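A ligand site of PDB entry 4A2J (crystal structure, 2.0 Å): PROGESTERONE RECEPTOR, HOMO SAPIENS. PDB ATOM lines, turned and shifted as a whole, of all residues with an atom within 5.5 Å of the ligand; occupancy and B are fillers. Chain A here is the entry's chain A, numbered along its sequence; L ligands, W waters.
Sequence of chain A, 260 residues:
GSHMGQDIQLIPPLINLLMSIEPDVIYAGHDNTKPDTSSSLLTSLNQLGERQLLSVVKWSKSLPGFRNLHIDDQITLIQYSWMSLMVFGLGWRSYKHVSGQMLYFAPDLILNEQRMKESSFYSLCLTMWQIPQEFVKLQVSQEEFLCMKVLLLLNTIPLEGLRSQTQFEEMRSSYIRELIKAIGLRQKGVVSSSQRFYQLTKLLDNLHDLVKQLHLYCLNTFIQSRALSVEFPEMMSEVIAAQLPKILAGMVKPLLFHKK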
ATOM      1  N   LEU A  42      16.047 -17.914   2.828  1.00  0.00           N
ATOM      2  CA  LEU A  42      16.572 -16.640   2.376  1.00  0.00           C
ATOM      3  C   LEU A  42      15.487 -15.563   2.467  1.00  0.00           C
ATOM      4  O   LEU A  42      15.793 -14.441   2.804  1.00  0.00           O
ATOM      5  CB  LEU A  42      17.179 -16.737   0.950  1.00  0.00           C
ATOM      6  CG  LEU A  42      18.510 -17.508   0.737  1.00  0.00           C
ATOM      7  CD1 LEU A  42      19.004 -17.323  -0.719  1.00  0.00           C
ATOM      8  CD2 LEU A  42      19.620 -17.122   1.693  1.00  0.00           C
ATOM      9  N   LEU A  45      15.255 -14.801   6.316  1.00  0.00           N
ATOM     10  CA  LEU A  45      16.430 -14.050   6.730  1.00  0.00           C
ATOM     11  C   LEU A  45      16.387 -12.577   6.265  1.00  0.00           C
ATOM     12  O   LEU A  45      16.792 -11.684   6.995  1.00  0.00           O
ATOM     13  CB  LEU A  45      17.722 -14.742   6.244  1.00  0.00           C
ATOM     14  CG  LEU A  45      18.217 -15.839   7.198  1.00  0.00           C
ATOM     15  CD1 LEU A  45      19.269 -16.706   6.546  1.00  0.00           C
ATOM     16  CD2 LEU A  45      18.754 -15.200   8.481  1.00  0.00           C
ATOM     17  N   ASN A  46      15.853 -12.333   5.070  1.00  0.00           N
ATOM     18  CA  ASN A  46      15.735 -10.969   4.549  1.00  0.00           C
ATOM     19  C   ASN A  46      14.654 -10.185   5.262  1.00  0.00           C
ATOM     20  O   ASN A  46      14.894  -9.083   5.700  1.00  0.00           O
ATOM     21  CB  ASN A  46      15.541 -10.963   3.038  1.00  0.00           C
ATOM     22  CG  ASN A  46      16.784 -11.419   2.278  1.00  0.00           C
ATOM     23  OD1 ASN A  46      17.876 -11.512   2.832  1.00  0.00           O
ATOM     24  ND2 ASN A  46      16.607 -11.697   0.990  1.00  0.00           N
ATOM     25  N   LEU A  48      13.679 -10.741   8.253  1.00  0.00           N
ATOM     26  CA  LEU A  48      14.238 -10.522   9.578  1.00  0.00           C
ATOM     27  C   LEU A  48      15.289  -9.413   9.558  1.00  0.00           C
ATOM     28  O   LEU A  48      15.315  -8.555  10.446  1.00  0.00           O
ATOM     29  CB  LEU A  48      14.818 -11.848  10.135  1.00  0.00           C
ATOM     30  CG  LEU A  48      15.619 -11.777  11.446  1.00  0.00           C
ATOM     31  CD1 LEU A  48      14.769 -11.214  12.577  1.00  0.00           C
ATOM     32  CD2 LEU A  48      16.175 -13.158  11.812  1.00  0.00           C
ATOM     33  N   GLY A  49      16.156  -9.441   8.566  1.00  0.00           N
ATOM     34  CA  GLY A  49      17.176  -8.431   8.425  1.00  0.00           C
ATOM     35  C   GLY A  49      16.594  -7.035   8.225  1.00  0.00           C
ATOM     36  O   GLY A  49      17.051  -6.096   8.866  1.00  0.00           O
ATOM     37  N   GLU A  50      15.574  -6.904   7.394  1.00  0.00           N
ATOM     38  CA  GLU A  50      14.859  -5.621   7.220  1.00  0.00           C
ATOM     39  C   GLU A  50      14.390  -5.060   8.578  1.00  0.00           C
ATOM     40  O   GLU A  50      14.615  -3.878   8.892  1.00  0.00           O
ATOM     41  CB  GLU A  50      13.667  -5.808   6.272  1.00  0.00           C
ATOM     42  CG  GLU A  50      12.960  -4.522   5.881  1.00  0.00           C
ATOM     43  CD  GLU A  50      13.688  -3.764   4.794  1.00  0.00           C
ATOM     44  OE1 GLU A  50      14.899  -4.011   4.571  1.00  0.00           O
ATOM     45  OE2 GLU A  50      13.038  -2.907   4.141  1.00  0.00           O
ATOM     46  N   GLN A  52      15.545  -6.036  11.631  1.00  0.00           N
ATOM     47  CA  GLN A  52      16.720  -5.698  12.441  1.00  0.00           C
ATOM     48  C   GLN A  52      17.346  -4.351  12.031  1.00  0.00           C
ATOM     49  O   GLN A  52      17.705  -3.552  12.902  1.00  0.00           O
ATOM     50  CB  GLN A  52      17.753  -6.821  12.438  1.00  0.00           C
ATOM     51  CG  GLN A  52      17.207  -8.108  13.024  1.00  0.00           C
ATOM     52  CD  GLN A  52      18.226  -9.222  13.090  1.00  0.00           C
ATOM     53  OE1 GLN A  52      19.375  -9.036  12.684  1.00  0.00           O
ATOM     54  NE2 GLN A  52      17.824 -10.384  13.594  1.00  0.00           N
ATOM     55  N   LEU A  53      17.453  -4.080  10.734  1.00  0.00           N
ATOM     56  CA  LEU A  53      18.009  -2.787  10.285  1.00  0.00           C
ATOM     57  C   LEU A  53      17.131  -1.599  10.682  1.00  0.00           C
ATOM     58  O   LEU A  53      17.654  -0.531  11.043  1.00  0.00           O
ATOM     59  CB  LEU A  53      18.225  -2.763   8.796  1.00  0.00           C
ATOM     60  CG  LEU A  53      18.915  -1.496   8.290  1.00  0.00           C
ATOM     61  CD1 LEU A  53      20.250  -1.304   9.039  1.00  0.00           C
ATOM     62  CD2 LEU A  53      19.123  -1.641   6.815  1.00  0.00           C
ATOM     63  N   TRP A  82      25.940  -1.752   8.373  1.00  0.00           N
ATOM     64  CA  TRP A  82      24.793  -2.634   8.690  1.00  0.00           C
ATOM     65  C   TRP A  82      25.125  -4.116   8.775  1.00  0.00           C
ATOM     66  O   TRP A  82      24.685  -4.797   9.717  1.00  0.00           O
ATOM     67  CB  TRP A  82      23.592  -2.422   7.738  1.00  0.00           C
ATOM     68  CG  TRP A  82      23.842  -2.741   6.281  1.00  0.00           C
ATOM     69  CD1 TRP A  82      24.298  -1.881   5.336  1.00  0.00           C
ATOM     70  CD2 TRP A  82      23.614  -4.001   5.612  1.00  0.00           C
ATOM     71  NE1 TRP A  82      24.392  -2.529   4.108  1.00  0.00           N
ATOM     72  CE2 TRP A  82      23.978  -3.828   4.257  1.00  0.00           C
ATOM     73  CE3 TRP A  82      23.160  -5.259   6.036  1.00  0.00           C
ATOM     74  CZ2 TRP A  82      23.864  -4.847   3.318  1.00  0.00           C
ATOM     75  CZ3 TRP A  82      23.062  -6.292   5.089  1.00  0.00           C
ATOM     76  CH2 TRP A  82      23.413  -6.078   3.751  1.00  0.00           C
ATOM     77  N   MET A  83      25.889  -4.641   7.827  1.00  0.00           N
ATOM     78  CA  MET A  83      26.186  -6.080   7.860  1.00  0.00           C
ATOM     79  C   MET A  83      27.002  -6.430   9.126  1.00  0.00           C
ATOM     80  O   MET A  83      26.757  -7.455   9.779  1.00  0.00           O
ATOM     81  CB  MET A  83      26.937  -6.508   6.599  1.00  0.00           C
ATOM     82  CG  MET A  83      27.253  -8.011   6.566  1.00  0.00           C
ATOM     83  SD  MET A  83      25.792  -8.938   6.071  1.00  0.00           S
ATOM     84  CE  MET A  83      25.755  -8.505   4.324  1.00  0.00           C
ATOM     85  N   MET A  86      24.781  -6.486  12.268  1.00  0.00           N
ATOM     86  CA  MET A  86      23.877  -7.635  12.386  1.00  0.00           C
ATOM     87  C   MET A  86      24.530  -8.987  12.634  1.00  0.00           C
ATOM     88  O   MET A  86      23.992  -9.788  13.379  1.00  0.00           O
ATOM     89  CB  MET A  86      22.980  -7.684  11.198  1.00  0.00           C
ATOM     90  CG  MET A  86      22.053  -6.527  11.316  1.00  0.00           C
ATOM     91  SD  MET A  86      20.916  -6.582  10.039  1.00  0.00           S
ATOM     92  CE  MET A  86      20.387  -4.874  10.127  1.00  0.00           C
ATOM     93  N   VAL A  87      25.693  -9.202  12.030  1.00  0.00           N
ATOM     94  CA  VAL A  87      26.438 -10.429  12.275  1.00  0.00           C
ATOM     95  C   VAL A  87      26.994 -10.409  13.708  1.00  0.00           C
ATOM     96  O   VAL A  87      27.055 -11.426  14.373  1.00  0.00           O
ATOM     97  CB  VAL A  87      27.525 -10.655  11.158  1.00  0.00           C
ATOM     98  CG1 VAL A  87      28.817  -9.910  11.464  1.00  0.00           C
ATOM     99  CG2 VAL A  87      27.787 -12.147  10.950  1.00  0.00           C
ATOM    100  N   LEU A  90      24.047 -11.070  15.887  1.00  0.00           N
ATOM    101  CA  LEU A  90      23.806 -12.504  15.753  1.00  0.00           C
ATOM    102  C   LEU A  90      24.737 -13.263  16.681  1.00  0.00           C
ATOM    103  O   LEU A  90      24.302 -14.155  17.442  1.00  0.00           O
ATOM    104  CB  LEU A  90      24.062 -12.949  14.312  1.00  0.00           C
ATOM    105  CG  LEU A  90      24.070 -14.452  14.013  1.00  0.00           C
ATOM    106  CD1 LEU A  90      22.733 -15.045  14.444  1.00  0.00           C
ATOM    107  CD2 LEU A  90      24.353 -14.678  12.559  1.00  0.00           C
ATOM    108  N   ARG A  93      23.668 -12.897  20.472  1.00  0.00           N
ATOM    109  CA  ARG A  93      22.489 -13.679  20.792  1.00  0.00           C
ATOM    110  C   ARG A  93      22.807 -15.180  20.869  1.00  0.00           C
ATOM    111  O   ARG A  93      22.313 -15.868  21.759  1.00  0.00           O
ATOM    112  CB  ARG A  93      21.388 -13.452  19.760  1.00  0.00           C
ATOM    113  CG  ARG A  93      20.750 -12.099  19.850  1.00  0.00           C
ATOM    114  CD  ARG A  93      19.510 -12.014  19.000  1.00  0.00           C
ATOM    115  NE  ARG A  93      19.779 -12.338  17.599  1.00  0.00           N
ATOM    116  CZ  ARG A  93      20.245 -11.470  16.694  1.00  0.00           C
ATOM    117  NH1 ARG A  93      20.497 -10.203  17.015  1.00  0.00           N
ATOM    118  NH2 ARG A  93      20.460 -11.877  15.448  1.00  0.00           N
ATOM    119  N   TYR A 104      21.519 -18.111  16.457  1.00  0.00           N
ATOM    120  CA  TYR A 104      20.283 -17.545  17.015  1.00  0.00           C
ATOM    121  C   TYR A 104      19.900 -16.281  16.245  1.00  0.00           C
ATOM    122  O   TYR A 104      20.102 -15.164  16.719  1.00  0.00           O
ATOM    123  CB  TYR A 104      20.467 -17.227  18.523  1.00  0.00           C
ATOM    124  CG  TYR A 104      19.175 -17.021  19.308  1.00  0.00           C
ATOM    125  CD1 TYR A 104      18.388 -15.884  19.121  1.00  0.00           C
ATOM    126  CD2 TYR A 104      18.759 -17.937  20.277  1.00  0.00           C
ATOM    127  CE1 TYR A 104      17.227 -15.681  19.831  1.00  0.00           C
ATOM    128  CE2 TYR A 104      17.582 -17.745  20.999  1.00  0.00           C
ATOM    129  CZ  TYR A 104      16.821 -16.604  20.769  1.00  0.00           C
ATOM    130  OH  TYR A 104      15.661 -16.372  21.457  1.00  0.00           O
ATOM    131  N   PHE A 105      19.399 -16.460  15.031  1.00  0.00           N
ATOM    132  CA  PHE A 105      18.972 -15.311  14.213  1.00  0.00           C
ATOM    133  C   PHE A 105      17.806 -14.630  14.901  1.00  0.00           C
ATOM    134  O   PHE A 105      17.808 -13.425  15.102  1.00  0.00           O
ATOM    135  CB  PHE A 105      18.592 -15.741  12.790  1.00  0.00           C
ATOM    136  CG  PHE A 105      19.735 -16.294  11.993  1.00  0.00           C
ATOM    137  CD1 PHE A 105      20.649 -15.455  11.401  1.00  0.00           C
ATOM    138  CD2 PHE A 105      19.882 -17.670  11.813  1.00  0.00           C
ATOM    139  CE1 PHE A 105      21.696 -15.952  10.645  1.00  0.00           C
ATOM    140  CE2 PHE A 105      20.945 -18.173  11.069  1.00  0.00           C
ATOM    141  CZ  PHE A 105      21.848 -17.313  10.482  1.00  0.00           C
ATOM    142  N   PHE A 121      23.553 -22.953   2.433  1.00  0.00           N
ATOM    143  CA  PHE A 121      24.692 -22.029   2.628  1.00  0.00           C
ATOM    144  C   PHE A 121      25.479 -22.415   3.879  1.00  0.00           C
ATOM    145  O   PHE A 121      25.872 -21.585   4.691  1.00  0.00           O
ATOM    146  CB  PHE A 121      24.240 -20.566   2.643  1.00  0.00           C
ATOM    147  CG  PHE A 121      22.985 -20.334   3.429  1.00  0.00           C
ATOM    148  CD1 PHE A 121      21.742 -20.631   2.879  1.00  0.00           C
ATOM    149  CD2 PHE A 121      23.038 -19.818   4.713  1.00  0.00           C
ATOM    150  CE1 PHE A 121      20.574 -20.428   3.612  1.00  0.00           C
ATOM    151  CE2 PHE A 121      21.877 -19.594   5.448  1.00  0.00           C
ATOM    152  CZ  PHE A 121      20.644 -19.912   4.893  1.00  0.00           C
ATOM    153  N   LEU A 124      28.662 -20.477   4.692  1.00  0.00           N
ATOM    154  CA  LEU A 124      28.308 -19.157   5.157  1.00  0.00           C
ATOM    155  C   LEU A 124      27.887 -19.254   6.614  1.00  0.00           C
ATOM    156  O   LEU A 124      28.297 -18.424   7.422  1.00  0.00           O
ATOM    157  CB  LEU A 124      27.185 -18.540   4.312  1.00  0.00           C
ATOM    158  CG  LEU A 124      27.100 -17.010   4.439  1.00  0.00           C
ATOM    159  CD1 LEU A 124      28.128 -16.370   3.525  1.00  0.00           C
ATOM    160  CD2 LEU A 124      25.709 -16.456   4.125  1.00  0.00           C
ATOM    161  N   MET A 128      29.830 -17.348   9.724  1.00  0.00           N
ATOM    162  CA  MET A 128      29.107 -16.581  10.716  1.00  0.00           C
ATOM    163  C   MET A 128      29.226 -17.158  12.124  1.00  0.00           C
ATOM    164  O   MET A 128      29.155 -16.420  13.090  1.00  0.00           O
ATOM    165  CB  MET A 128      27.647 -16.459  10.306  1.00  0.00           C
ATOM    166  CG  MET A 128      27.422 -15.583   9.094  1.00  0.00           C
ATOM    167  SD  MET A 128      25.673 -15.253   8.845  1.00  0.00           S
ATOM    168  CE  MET A 128      25.050 -16.866   8.373  1.00  0.00           C
ATOM    169  N   LEU A 214      30.541 -11.897   3.598  1.00  0.00           N
ATOM    170  CA  LEU A 214      29.068 -11.795   3.662  1.00  0.00           C
ATOM    171  C   LEU A 214      28.557 -10.782   2.625  1.00  0.00           C
ATOM    172  O   LEU A 214      27.537 -11.013   1.986  1.00  0.00           O
ATOM    173  CB  LEU A 214      28.595 -11.415   5.072  1.00  0.00           C
ATOM    174  CG  LEU A 214      29.113 -12.201   6.284  1.00  0.00           C
ATOM    175  CD1 LEU A 214      28.313 -11.804   7.541  1.00  0.00           C
ATOM    176  CD2 LEU A 214      29.078 -13.683   6.096  1.00  0.00           C
ATOM    177  N   TYR A 217      28.662 -12.582  -0.797  1.00  0.00           N
ATOM    178  CA  TYR A 217      27.518 -13.496  -0.838  1.00  0.00           C
ATOM    179  C   TYR A 217      26.212 -12.732  -1.045  1.00  0.00           C
ATOM    180  O   TYR A 217      25.368 -13.097  -1.856  1.00  0.00           O
ATOM    181  CB  TYR A 217      27.412 -14.318   0.452  1.00  0.00           C
ATOM    182  CG  TYR A 217      26.434 -15.462   0.306  1.00  0.00           C
ATOM    183  CD1 TYR A 217      25.070 -15.278   0.519  1.00  0.00           C
ATOM    184  CD2 TYR A 217      26.869 -16.730  -0.071  1.00  0.00           C
ATOM    185  CE1 TYR A 217      24.169 -16.314   0.362  1.00  0.00           C
ATOM    186  CE2 TYR A 217      25.968 -17.790  -0.223  1.00  0.00           C
ATOM    187  CZ  TYR A 217      24.620 -17.574   0.003  1.00  0.00           C
ATOM    188  OH  TYR A 217      23.704 -18.597  -0.146  1.00  0.00           O
ATOM    189  N   CYS A 218      26.061 -11.652  -0.299  1.00  0.00           N
ATOM    190  CA  CYS A 218      24.825 -10.914  -0.310  1.00  0.00           C
ATOM    191  C   CYS A 218      24.605 -10.334  -1.694  1.00  0.00           C
ATOM    192  O   CYS A 218      23.563 -10.564  -2.306  1.00  0.00           O
ATOM    193  CB  CYS A 218      24.838  -9.835   0.774  1.00  0.00           C
ATOM    194  SG  CYS A 218      23.444  -8.710   0.656  1.00  0.00           S
ATOM    195  N   THR A 221      23.739 -12.943  -4.345  1.00  0.00           N
ATOM    196  CA  THR A 221      22.358 -13.406  -4.160  1.00  0.00           C
ATOM    197  C   THR A 221      21.369 -12.339  -4.639  1.00  0.00           C
ATOM    198  O   THR A 221      20.326 -12.670  -5.215  1.00  0.00           O
ATOM    199  CB  THR A 221      22.056 -13.802  -2.671  1.00  0.00           C
ATOM    200  OG1 THR A 221      22.986 -14.776  -2.226  1.00  0.00           O
ATOM    201  CG2 THR A 221      20.658 -14.401  -2.543  1.00  0.00           C
ATOM    202  N   PHE A 232      13.941  -9.400  -1.873  1.00  0.00           N
ATOM    203  CA  PHE A 232      14.791  -8.411  -1.256  1.00  0.00           C
ATOM    204  C   PHE A 232      13.921  -7.203  -0.925  1.00  0.00           C
ATOM    205  O   PHE A 232      13.373  -6.584  -1.821  1.00  0.00           O
ATOM    206  CB  PHE A 232      15.992  -8.101  -2.153  1.00  0.00           C
ATOM    207  CG  PHE A 232      17.061  -9.168  -2.109  1.00  0.00           C
ATOM    208  CD1 PHE A 232      16.838 -10.414  -2.663  1.00  0.00           C
ATOM    209  CD2 PHE A 232      18.268  -8.947  -1.454  1.00  0.00           C
ATOM    210  CE1 PHE A 232      17.785 -11.412  -2.588  1.00  0.00           C
ATOM    211  CE2 PHE A 232      19.235  -9.956  -1.374  1.00  0.00           C
ATOM    212  CZ  PHE A 232      18.994 -11.185  -1.950  1.00  0.00           C
ATOM    213  N   PRO A 233      13.737  -6.919   0.390  1.00  0.00           N
ATOM    214  CA  PRO A 233      12.993  -5.768   0.903  1.00  0.00           C
ATOM    215  C   PRO A 233      13.526  -4.390   0.472  1.00  0.00           C
ATOM    216  O   PRO A 233      14.692  -4.253   0.071  1.00  0.00           O
ATOM    217  CB  PRO A 233      13.135  -5.918   2.412  1.00  0.00           C
ATOM    218  CG  PRO A 233      13.248  -7.311   2.636  1.00  0.00           C
ATOM    219  CD  PRO A 233      14.031  -7.865   1.474  1.00  0.00           C
ATOM    220  N   MET A 235      14.318  -1.409   2.102  1.00  0.00           N
ATOM    221  CA  MET A 235      15.499  -0.795   2.706  1.00  0.00           C
ATOM    222  C   MET A 235      16.752  -1.608   2.372  1.00  0.00           C
ATOM    223  O   MET A 235      17.817  -1.031   2.145  1.00  0.00           O
ATOM    224  CB  MET A 235      15.350  -0.635   4.231  1.00  0.00           C
ATOM    225  CG  MET A 235      16.529   0.145   4.832  1.00  0.00           C
ATOM    226  SD  MET A 235      16.305   0.667   6.576  1.00  0.00           S
ATOM    227  CE  MET A 235      14.610   1.265   6.497  1.00  0.00           C
ATOM    228  N   MET A 236      16.614  -2.929   2.361  1.00  0.00           N
ATOM    229  CA  MET A 236      17.731  -3.819   2.010  1.00  0.00           C
ATOM    230  C   MET A 236      18.249  -3.476   0.612  1.00  0.00           C
ATOM    231  O   MET A 236      19.445  -3.276   0.399  1.00  0.00           O
ATOM    232  CB  MET A 236      17.282  -5.281   2.029  1.00  0.00           C
ATOM    233  CG  MET A 236      18.451  -6.258   2.060  1.00  0.00           C
ATOM    234  SD  MET A 236      17.880  -7.910   1.784  1.00  0.00           S
ATOM    235  CE  MET A 236      19.447  -8.823   1.905  1.00  0.00           C
ATOM    236  N   VAL A 239      20.089  -0.003   0.656  1.00  0.00           N
ATOM    237  CA  VAL A 239      21.461   0.012   1.202  1.00  0.00           C
ATOM    238  C   VAL A 239      22.443  -0.736   0.298  1.00  0.00           C
ATOM    239  O   VAL A 239      23.620  -0.358   0.187  1.00  0.00           O
ATOM    240  CB  VAL A 239      21.560  -0.516   2.671  1.00  0.00           C
ATOM    241  CG1 VAL A 239      20.760   0.392   3.625  1.00  0.00           C
ATOM    242  CG2 VAL A 239      21.126  -2.018   2.784  1.00  0.00           C
HETATM  243  C1  LIG L   1      22.422 -16.533   3.918  1.00  0.00           C
HETATM  244  C2  LIG L   1      22.014 -14.257   3.327  1.00  0.00           C
HETATM  245  C3  LIG L   1      22.707 -12.877   3.369  1.00  0.00           C
HETATM  246  C4  LIG L   1      24.228 -13.065   3.645  1.00  0.00           C
HETATM  247  C5  LIG L   1      24.481 -12.635   5.106  1.00  0.00           C
HETATM  248  O1  LIG L   1      22.560 -15.153   4.295  1.00  0.00           O
HETATM  249  C6  LIG L   1      23.071 -12.505   5.705  1.00  0.00           C
HETATM  250  C7  LIG L   1      22.996 -11.591   6.933  1.00  0.00           C
HETATM  251  C8  LIG L   1      23.798 -12.249   8.027  1.00  0.00           C
HETATM  252  C9  LIG L   1      23.656 -11.474   9.337  1.00  0.00           C
HETATM  253  C10 LIG L   1      22.197 -11.492   9.718  1.00  0.00           C
HETATM  254  C11 LIG L   1      21.851 -11.621  11.023  1.00  0.00           C
HETATM  255  C12 LIG L   1      20.511 -11.752  11.391  1.00  0.00           C
HETATM  256  O2  LIG L   1      20.219 -11.969  12.559  1.00  0.00           O
HETATM  257  C13 LIG L   1      19.380 -11.691  10.401  1.00  0.00           C
HETATM  258  C14 LIG L   1      19.753 -11.061   9.062  1.00  0.00           C
HETATM  259  C15 LIG L   1      21.190 -11.358   8.646  1.00  0.00           C
HETATM  260  C16 LIG L   1      21.553 -11.408   7.336  1.00  0.00           C
HETATM  261  C17 LIG L   1      20.489 -11.247   6.265  1.00  0.00           C
HETATM  262  C18 LIG L   1      20.781 -11.945   4.926  1.00  0.00           C
HETATM  263  C19 LIG L   1      22.254 -11.939   4.506  1.00  0.00           C
HETATM  264  C20 LIG L   1      22.639 -10.516   4.125  1.00  0.00           C
HETATM  265  C21 LIG L   1      20.096  -9.771   6.152  1.00  0.00           C
HETATM  266  C22 LIG L   1      20.769  -8.743   6.818  1.00  0.00           C
HETATM  267  C23 LIG L   1      20.344  -7.424   6.737  1.00  0.00           C
HETATM  268  C24 LIG L   1      19.238  -7.103   5.948  1.00  0.00           C
HETATM  269  C25 LIG L   1      18.768  -5.705   5.891  1.00  0.00           C
HETATM  270  N1  LIG L   1      17.620  -5.448   5.333  1.00  0.00           N
HETATM  271  O3  LIG L   1      17.174  -4.108   5.334  1.00  0.00           O
HETATM  272  C26 LIG L   1      18.543  -8.138   5.288  1.00  0.00           C
HETATM  273  C27 LIG L   1      18.982  -9.455   5.402  1.00  0.00           C
HETATM  274  O4  LIG L   1      22.637 -12.294   2.067  1.00  0.00           O
HETATM  275  C28 LIG L   1      21.347 -12.198   1.427  1.00  0.00           C
HETATM  276  O   HOH W   1      21.492  -9.248  14.213  1.00  0.00           O
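N1 of the ligand lies within hydrogen-bond range of N of Glu 50, at 3.2 Å. An oxygen (O2) of the ligand is in hydrogen-bond range of the guanidinium group of Arg 93 (2.9 Å). The side-chain amide nitrogen (NE2) of Gln 52 lies within hydrogen-bond range of an oxygen (O2) of the ligand. O3 of the ligand sits at hydrogen-bond distance from OE1 of Glu 50. O3 of the ligand sits at hydrogen-bond distance from N of Met 236, at 3.2 Å.
The side-chain carboxylate (OE2) of Glu 50 is in hydrogen-bond range of the backbone NH (N) of Met 235 (2.8 Å). The side-chain sulfur (SD) of Met 236 lies close to the side-chain amide oxygen (OD1) of Asn 46 (3.8 Å). The side-chain carboxylate of Glu 50 sits at hydrogen-bond distance from the backbone NH of Met 236, at 3.0 Å. The side-chain amide nitrogen (NE2) of Gln 52 is in hydrogen-bond range of the backbone carbonyl oxygen (O) of Phe 105 (3.4 Å). The backbone carbonyl oxygen (O) of Tyr 104 sits at hydrogen-bond distance from the guanidinium group (NE) of Arg 93, 3.0 Å away. ND2 of Asn 46 lies close to O of Leu 42 (3.4 Å). The backbone carbonyl oxygen (O) of Tyr 217 sits at hydrogen-bond distance from the side-chain hydroxyl (OG1) of Thr 221, 2.9 Å away. NH2 of Arg 93 lies within hydrogen-bond range of O of Phe 105 (3.1 Å).
Leu 42 touches the ligand. O of Leu 45 touches C27 of the ligand, at 3.5 Å. Asn 46 touches the ligand. Leu 48 touches the ligand (CD2 to C13, 3.8 Å). Gly 49 touches the ligand. Leu 53 touches the ligand. Trp 82 touches the ligand. Met 83 touches the ligand. Met 86 touches the ligand (SD to C23, 3.5 Å). Phe 105 touches the ligand. Phe 121 touches the ligand. CD2 of Leu 124 touches C1 of the ligand, at 3.3 Å. Met 128 touches the ligand (SD to C8, 3.6 Å). Tyr 217 touches the ligand. Cys 218 touches the ligand (CA to O4, 3.5 Å). C of Met 235 touches O3 of the ligand (3.9 Å). Hydrophobic or aromatic side chains that line the ligand: Leu 42, Leu 48, Leu 53, Trp 82, Met 83, Met 86, Phe 105, Phe 121, Leu 124, Met 128, Tyr 217 and Met 236. The nearest printed residue that does not touch the ligand is Val 87 (4.1 Å).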
